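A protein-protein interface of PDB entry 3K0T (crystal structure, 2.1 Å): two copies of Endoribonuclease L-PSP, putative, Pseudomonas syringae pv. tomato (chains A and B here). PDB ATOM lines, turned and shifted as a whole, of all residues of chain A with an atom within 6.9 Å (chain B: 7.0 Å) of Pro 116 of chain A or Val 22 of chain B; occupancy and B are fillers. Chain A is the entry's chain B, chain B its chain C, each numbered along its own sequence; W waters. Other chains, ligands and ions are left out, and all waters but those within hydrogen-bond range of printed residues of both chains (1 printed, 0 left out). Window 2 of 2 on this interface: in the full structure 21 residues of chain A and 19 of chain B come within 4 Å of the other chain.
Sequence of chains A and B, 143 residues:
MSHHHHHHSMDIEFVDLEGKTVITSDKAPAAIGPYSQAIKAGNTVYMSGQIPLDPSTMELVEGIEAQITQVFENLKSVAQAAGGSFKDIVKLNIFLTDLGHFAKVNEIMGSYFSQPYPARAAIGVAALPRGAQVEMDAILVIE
Of chain B, only Lys 20 and Val 22 come within 4 Å of Pro 116 of chain A.
Val 22 of chain B touches one residue of chain A.
Printed residues of chain B within 4 Å of Tyr 117 of chain A: Tyr 35 (3.4 Å), Ser 36 (2.6 Å) and Ile 39 (3.2 Å).
Of the printed residues of chain A, Tyr 35 of chain B touches Tyr 117 (3.4 Å) and Pro 118 (3.1 Å).
Of the printed residues of chain B, Ile 89 of chain A touches Lys 20.
The nearest residue of chain B that does not touch Pro 116 of chain A is Ser 36 of chain B (4.5 Å).
The nearest residue of chain A that does not touch Val 22 of chain B is Tyr 117 of chain A (5.0 Å).
Printed residues of chain B that touch a printed residue of chain A: Lys 20, Val 22, Tyr 35, Ser 36 and Ile 39.
Hydrophobic or aromatic side chains of chain B within 4 Å of the printed part of chain A: Val 22, Tyr 35 and Ile 39.
Hydrophobic or aromatic side chains of chain A within 4 Å of the printed part of chain B: Pro 116 and Tyr 117.
Along chain A the printed residues that touch a printed residue of chain B span positions 87 to 118.
Among the printed residues, 9 pairs touch across the chains.
Among the printed residues, no Asp or Glu carboxylate lies within 4 Å of a Lys or Arg side-chain nitrogen of the other chain.
Water W1 lies within hydrogen-bond range of O of Pro 116 of chain A, NZ of Lys 20 of chain B and O of Lys 87 of chain A.
O of Lys 87 of chain A sits at hydrogen-bond distance from NZ of Lys 20 of chain B (3.3 Å).
The backbone carbonyl oxygen of Tyr 117 of chain A is in hydrogen-bond range of the side-chain hydroxyl of Ser 36 of chain B, 2.6 Å away.
The backbone carbonyl oxygen (O) of Pro 118 of chain A sits at hydrogen-bond distance from the backbone NH (N) of Ser 36 of chain B, at 3.0 Å.
Among the printed residues, pairs that only touch across the chains: Pro 118 of chain A with Tyr 35 of chain B, Tyr 117 of chain A with Ile 39 of chain B, Pro 116 of chain A with Val 22 of chain B, Tyr 117 of chain A with Tyr 35 of chain B, Pro 116 of chain A with Lys 20 of chain B and Ile 89 of chain A with Lys 20 of chain B.
No position is printed for both chains.
Of the 9 pairs that touch across the chains among the printed residues, none has its exchanged pair printed and touching as well.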
ATOM      1  N   PHE A  86       0.213 -24.149  -6.657  1.00  0.00           N
ATOM      2  CA  PHE A  86      -1.099 -24.643  -7.082  1.00  0.00           C
ATOM      3  C   PHE A  86      -1.911 -25.249  -5.926  1.00  0.00           C
ATOM      4  O   PHE A  86      -3.143 -25.260  -5.966  1.00  0.00           O
ATOM      5  CB  PHE A  86      -0.934 -25.636  -8.249  1.00  0.00           C
ATOM      6  CG  PHE A  86      -0.878 -24.975  -9.619  1.00  0.00           C
ATOM      7  CD1 PHE A  86      -0.715 -23.596  -9.739  1.00  0.00           C
ATOM      8  CD2 PHE A  86      -1.006 -25.734 -10.786  1.00  0.00           C
ATOM      9  CE1 PHE A  86      -0.665 -22.979 -10.996  1.00  0.00           C
ATOM     10  CE2 PHE A  86      -0.957 -25.124 -12.053  1.00  0.00           C
ATOM     11  CZ  PHE A  86      -0.793 -23.742 -12.151  1.00  0.00           C
ATOM     12  N   LYS A  87      -1.219 -25.728  -4.895  1.00  0.00           N
ATOM     13  CA  LYS A  87      -1.872 -26.283  -3.710  1.00  0.00           C
ATOM     14  C   LYS A  87      -2.710 -25.228  -2.988  1.00  0.00           C
ATOM     15  O   LYS A  87      -3.667 -25.564  -2.287  1.00  0.00           O
ATOM     16  CB  LYS A  87      -0.829 -26.827  -2.721  1.00  0.00           C
ATOM     17  CG  LYS A  87      -0.203 -28.146  -3.116  1.00  0.00           C
ATOM     18  CD  LYS A  87       0.921 -28.529  -2.150  1.00  0.00           C
ATOM     19  CE  LYS A  87       1.309 -29.993  -2.314  1.00  0.00           C
ATOM     20  NZ  LYS A  87       1.884 -30.282  -3.659  1.00  0.00           N
ATOM     21  N   ILE A  89      -4.346 -22.732  -4.556  1.00  0.00           N
ATOM     22  CA  ILE A  89      -5.427 -22.231  -5.401  1.00  0.00           C
ATOM     23  C   ILE A  89      -6.755 -22.757  -4.880  1.00  0.00           C
ATOM     24  O   ILE A  89      -6.918 -23.957  -4.684  1.00  0.00           O
ATOM     25  CB  ILE A  89      -5.221 -22.638  -6.883  1.00  0.00           C
ATOM     26  CG1 ILE A  89      -4.131 -21.757  -7.505  1.00  0.00           C
ATOM     27  CG2 ILE A  89      -6.531 -22.497  -7.671  1.00  0.00           C
ATOM     28  CD1 ILE A  89      -3.704 -22.159  -8.909  1.00  0.00           C
ATOM     29  N   PHE A 113      -2.518 -30.635 -10.394  1.00  0.00           N
ATOM     30  CA  PHE A 113      -3.158 -30.514  -9.087  1.00  0.00           C
ATOM     31  C   PHE A 113      -3.393 -31.887  -8.471  1.00  0.00           C
ATOM     32  O   PHE A 113      -3.495 -32.882  -9.184  1.00  0.00           O
ATOM     33  CB  PHE A 113      -4.537 -29.828  -9.209  1.00  0.00           C
ATOM     34  CG  PHE A 113      -4.490 -28.403  -9.705  1.00  0.00           C
ATOM     35  CD1 PHE A 113      -4.572 -27.341  -8.814  1.00  0.00           C
ATOM     36  CD2 PHE A 113      -4.385 -28.123 -11.067  1.00  0.00           C
ATOM     37  CE1 PHE A 113      -4.560 -26.018  -9.266  1.00  0.00           C
ATOM     38  CE2 PHE A 113      -4.372 -26.803 -11.530  1.00  0.00           C
ATOM     39  CZ  PHE A 113      -4.458 -25.750 -10.624  1.00  0.00           C
ATOM     40  N   SER A 114      -3.492 -31.924  -7.144  1.00  0.00           N
ATOM     41  CA  SER A 114      -3.812 -33.148  -6.399  1.00  0.00           C
ATOM     42  C   SER A 114      -4.739 -32.714  -5.262  1.00  0.00           C
ATOM     43  O   SER A 114      -4.877 -31.516  -5.000  1.00  0.00           O
ATOM     44  CB  SER A 114      -2.542 -33.831  -5.856  1.00  0.00           C
ATOM     45  OG  SER A 114      -1.693 -32.912  -5.181  1.00  0.00           O
ATOM     46  N   GLN A 115      -5.391 -33.674  -4.614  1.00  0.00           N
ATOM     47  CA  GLN A 115      -6.305 -33.381  -3.509  1.00  0.00           C
ATOM     48  C   GLN A 115      -5.618 -32.623  -2.382  1.00  0.00           C
ATOM     49  O   GLN A 115      -4.458 -32.891  -2.072  1.00  0.00           O
ATOM     50  CB  GLN A 115      -6.877 -34.679  -2.931  1.00  0.00           C
ATOM     51  CG  GLN A 115      -7.903 -35.380  -3.792  1.00  0.00           C
ATOM     52  CD  GLN A 115      -8.713 -36.372  -2.985  1.00  0.00           C
ATOM     53  OE1 GLN A 115      -8.700 -37.574  -3.255  1.00  0.00           O
ATOM     54  NE2 GLN A 115      -9.416 -35.873  -1.968  1.00  0.00           N
ATOM     55  N   PRO A 116      -6.308 -31.646  -1.768  1.00  0.00           N
ATOM     56  CA  PRO A 116      -7.674 -31.205  -2.076  1.00  0.00           C
ATOM     57  C   PRO A 116      -7.694 -30.332  -3.343  1.00  0.00           C
ATOM     58  O   PRO A 116      -6.955 -29.352  -3.447  1.00  0.00           O
ATOM     59  CB  PRO A 116      -8.097 -30.448  -0.815  1.00  0.00           C
ATOM     60  CG  PRO A 116      -6.811 -29.948  -0.233  1.00  0.00           C
ATOM     61  CD  PRO A 116      -5.791 -31.025  -0.533  1.00  0.00           C
ATOM     62  N   TYR A 117      -8.524 -30.713  -4.310  1.00  0.00           N
ATOM     63  CA  TYR A 117      -8.646 -29.980  -5.575  1.00  0.00           C
ATOM     64  C   TYR A 117      -9.390 -28.657  -5.411  1.00  0.00           C
ATOM     65  O   TYR A 117     -10.256 -28.530  -4.552  1.00  0.00           O
ATOM     66  CB  TYR A 117      -9.394 -30.822  -6.598  1.00  0.00           C
ATOM     67  CG  TYR A 117      -8.662 -32.053  -7.059  1.00  0.00           C
ATOM     68  CD1 TYR A 117      -7.456 -31.955  -7.756  1.00  0.00           C
ATOM     69  CD2 TYR A 117      -9.193 -33.324  -6.821  1.00  0.00           C
ATOM     70  CE1 TYR A 117      -6.792 -33.099  -8.212  1.00  0.00           C
ATOM     71  CE2 TYR A 117      -8.542 -34.470  -7.271  1.00  0.00           C
ATOM     72  CZ  TYR A 117      -7.347 -34.352  -7.962  1.00  0.00           C
ATOM     73  OH  TYR A 117      -6.713 -35.493  -8.398  1.00  0.00           O
ATOM     74  N   PRO A 118      -9.071 -27.660  -6.248  1.00  0.00           N
ATOM     75  CA  PRO A 118      -9.779 -26.390  -6.096  1.00  0.00           C
ATOM     76  C   PRO A 118     -11.202 -26.422  -6.644  1.00  0.00           C
ATOM     77  O   PRO A 118     -11.588 -27.356  -7.354  1.00  0.00           O
ATOM     78  CB  PRO A 118      -8.891 -25.415  -6.866  1.00  0.00           C
ATOM     79  CG  PRO A 118      -8.326 -26.260  -7.969  1.00  0.00           C
ATOM     80  CD  PRO A 118      -8.081 -27.617  -7.344  1.00  0.00           C
ATOM     81  N   LYS B  20      -8.189 -24.281   5.432  1.00  0.00           N
ATOM     82  CA  LYS B  20      -8.878 -24.659   4.164  1.00  0.00           C
ATOM     83  C   LYS B  20      -9.635 -25.971   4.360  1.00  0.00           C
ATOM     84  O   LYS B  20      -9.141 -26.896   5.015  1.00  0.00           O
ATOM     85  CB  LYS B  20      -7.861 -24.773   3.021  1.00  0.00           C
ATOM     86  CG  LYS B  20      -8.443 -25.278   1.708  1.00  0.00           C
ATOM     87  CD  LYS B  20      -7.427 -25.205   0.557  1.00  0.00           C
ATOM     88  CE  LYS B  20      -7.782 -26.218  -0.534  1.00  0.00           C
ATOM     89  NZ  LYS B  20      -6.769 -26.323  -1.636  1.00  0.00           N
ATOM     90  N   THR B  21     -10.836 -26.044   3.789  1.00  0.00           N
ATOM     91  CA  THR B  21     -11.698 -27.209   3.944  1.00  0.00           C
ATOM     92  C   THR B  21     -12.411 -27.556   2.640  1.00  0.00           C
ATOM     93  O   THR B  21     -12.947 -26.676   1.969  1.00  0.00           O
ATOM     94  CB  THR B  21     -12.789 -26.922   5.013  1.00  0.00           C
ATOM     95  OG1 THR B  21     -12.161 -26.482   6.221  1.00  0.00           O
ATOM     96  CG2 THR B  21     -13.613 -28.164   5.302  1.00  0.00           C
ATOM     97  N   VAL B  22     -12.419 -28.838   2.288  1.00  0.00           N
ATOM     98  CA  VAL B  22     -13.140 -29.286   1.104  1.00  0.00           C
ATOM     99  C   VAL B  22     -14.589 -29.458   1.531  1.00  0.00           C
ATOM    100  O   VAL B  22     -14.867 -30.065   2.569  1.00  0.00           O
ATOM    101  CB  VAL B  22     -12.644 -30.658   0.574  1.00  0.00           C
ATOM    102  CG1 VAL B  22     -13.645 -31.206  -0.443  1.00  0.00           C
ATOM    103  CG2 VAL B  22     -11.285 -30.520  -0.074  1.00  0.00           C
ATOM    104  N   ILE B  23     -15.503 -28.908   0.740  1.00  0.00           N
ATOM    105  CA  ILE B  23     -16.923 -29.037   1.027  1.00  0.00           C
ATOM    106  C   ILE B  23     -17.488 -30.059   0.046  1.00  0.00           C
ATOM    107  O   ILE B  23     -17.275 -29.957  -1.172  1.00  0.00           O
ATOM    108  CB  ILE B  23     -17.683 -27.693   0.843  1.00  0.00           C
ATOM    109  CG1 ILE B  23     -17.011 -26.567   1.647  1.00  0.00           C
ATOM    110  CG2 ILE B  23     -19.147 -27.864   1.231  1.00  0.00           C
ATOM    111  CD1 ILE B  23     -16.804 -26.855   3.135  1.00  0.00           C
ATOM    112  N   THR B  24     -18.178 -31.060   0.584  1.00  0.00           N
ATOM    113  CA  THR B  24     -18.793 -32.086  -0.241  1.00  0.00           C
ATOM    114  C   THR B  24     -20.169 -32.391   0.311  1.00  0.00           C
ATOM    115  O   THR B  24     -20.324 -32.696   1.499  1.00  0.00           O
ATOM    116  CB  THR B  24     -18.008 -33.418  -0.246  1.00  0.00           C
ATOM    117  OG1 THR B  24     -16.623 -33.162  -0.508  1.00  0.00           O
ATOM    118  CG2 THR B  24     -18.559 -34.344  -1.329  1.00  0.00           C
ATOM    119  N   TYR B  35     -11.441 -31.289  -9.312  1.00  0.00           N
ATOM    120  CA  TYR B  35     -12.073 -30.148  -8.654  1.00  0.00           C
ATOM    121  C   TYR B  35     -12.878 -30.625  -7.452  1.00  0.00           C
ATOM    122  O   TYR B  35     -13.126 -31.817  -7.306  1.00  0.00           O
ATOM    123  CB  TYR B  35     -12.998 -29.372  -9.609  1.00  0.00           C
ATOM    124  CG  TYR B  35     -14.268 -30.093 -10.023  1.00  0.00           C
ATOM    125  CD1 TYR B  35     -15.523 -29.711  -9.529  1.00  0.00           C
ATOM    126  CD2 TYR B  35     -14.214 -31.136 -10.937  1.00  0.00           C
ATOM    127  CE1 TYR B  35     -16.695 -30.361  -9.951  1.00  0.00           C
ATOM    128  CE2 TYR B  35     -15.365 -31.787 -11.360  1.00  0.00           C
ATOM    129  CZ  TYR B  35     -16.599 -31.400 -10.869  1.00  0.00           C
ATOM    130  OH  TYR B  35     -17.725 -32.065 -11.309  1.00  0.00           O
ATOM    131  N   SER B  36     -13.255 -29.684  -6.589  1.00  0.00           N
ATOM    132  CA  SER B  36     -14.080 -29.966  -5.415  1.00  0.00           C
ATOM    133  C   SER B  36     -15.354 -29.159  -5.615  1.00  0.00           C
ATOM    134  O   SER B  36     -15.335 -28.147  -6.328  1.00  0.00           O
ATOM    135  CB  SER B  36     -13.391 -29.493  -4.128  1.00  0.00           C
ATOM    136  OG  SER B  36     -12.175 -30.185  -3.870  1.00  0.00           O
ATOM    137  N   GLN B  37     -16.455 -29.585  -4.994  1.00  0.00           N
ATOM    138  CA  GLN B  37     -17.713 -28.844  -5.126  1.00  0.00           C
ATOM    139  C   GLN B  37     -17.544 -27.403  -4.611  1.00  0.00           C
ATOM    140  O   GLN B  37     -18.094 -26.464  -5.185  1.00  0.00           O
ATOM    141  CB  GLN B  37     -18.838 -29.563  -4.370  1.00  0.00           C
ATOM    142  CG  GLN B  37     -19.183 -30.952  -4.930  1.00  0.00           C
ATOM    143  CD  GLN B  37     -20.187 -31.683  -4.056  1.00  0.00           C
ATOM    144  OE1 GLN B  37     -20.515 -31.223  -2.963  1.00  0.00           O
ATOM    145  NE2 GLN B  37     -20.678 -32.823  -4.531  1.00  0.00           N
ATOM    146  N   ALA B  38     -16.781 -27.240  -3.530  1.00  0.00           N
ATOM    147  CA  ALA B  38     -16.479 -25.921  -2.975  1.00  0.00           C
ATOM    148  C   ALA B  38     -15.259 -25.994  -2.070  1.00  0.00           C
ATOM    149  O   ALA B  38     -14.906 -27.068  -1.577  1.00  0.00           O
ATOM    150  CB  ALA B  38     -17.680 -25.361  -2.183  1.00  0.00           C
ATOM    151  N   ILE B  39     -14.615 -24.847  -1.879  1.00  0.00           N
ATOM    152  CA  ILE B  39     -13.468 -24.745  -0.988  1.00  0.00           C
ATOM    153  C   ILE B  39     -13.742 -23.595  -0.032  1.00  0.00           C
ATOM    154  O   ILE B  39     -14.059 -22.477  -0.455  1.00  0.00           O
ATOM    155  CB  ILE B  39     -12.132 -24.429  -1.727  1.00  0.00           C
ATOM    156  CG1 ILE B  39     -11.760 -25.553  -2.704  1.00  0.00           C
ATOM    157  CG2 ILE B  39     -11.004 -24.219  -0.695  1.00  0.00           C
ATOM    158  CD1 ILE B  39     -11.245 -26.827  -2.037  1.00  0.00           C
ATOM    159  N   LYS B  40     -13.643 -23.887   1.259  1.00  0.00           N
ATOM    160  CA  LYS B  40     -13.831 -22.870   2.268  1.00  0.00           C
ATOM    161  C   LYS B  40     -12.445 -22.481   2.744  1.00  0.00           C
ATOM    162  O   LYS B  40     -11.682 -23.332   3.178  1.00  0.00           O
ATOM    163  CB  LYS B  40     -14.669 -23.407   3.443  1.00  0.00           C
ATOM    164  CG  LYS B  40     -14.707 -22.471   4.656  1.00  0.00           C
ATOM    165  CD  LYS B  40     -15.680 -22.967   5.718  1.00  0.00           C
ATOM    166  CE  LYS B  40     -15.560 -22.157   7.004  1.00  0.00           C
ATOM    167  NZ  LYS B  40     -14.173 -22.254   7.585  1.00  0.00           N
ATOM    168  N   ALA B  81     -23.732 -27.751   3.060  1.00  0.00           N
ATOM    169  CA  ALA B  81     -22.621 -28.569   3.533  1.00  0.00           C
ATOM    170  C   ALA B  81     -21.440 -27.691   3.971  1.00  0.00           C
ATOM    171  O   ALA B  81     -20.569 -28.134   4.724  1.00  0.00           O
ATOM    172  CB  ALA B  81     -22.187 -29.552   2.450  1.00  0.00           C
HETATM  173  O   HOH W   1      -4.776 -28.178  -2.375  1.00  0.00           O
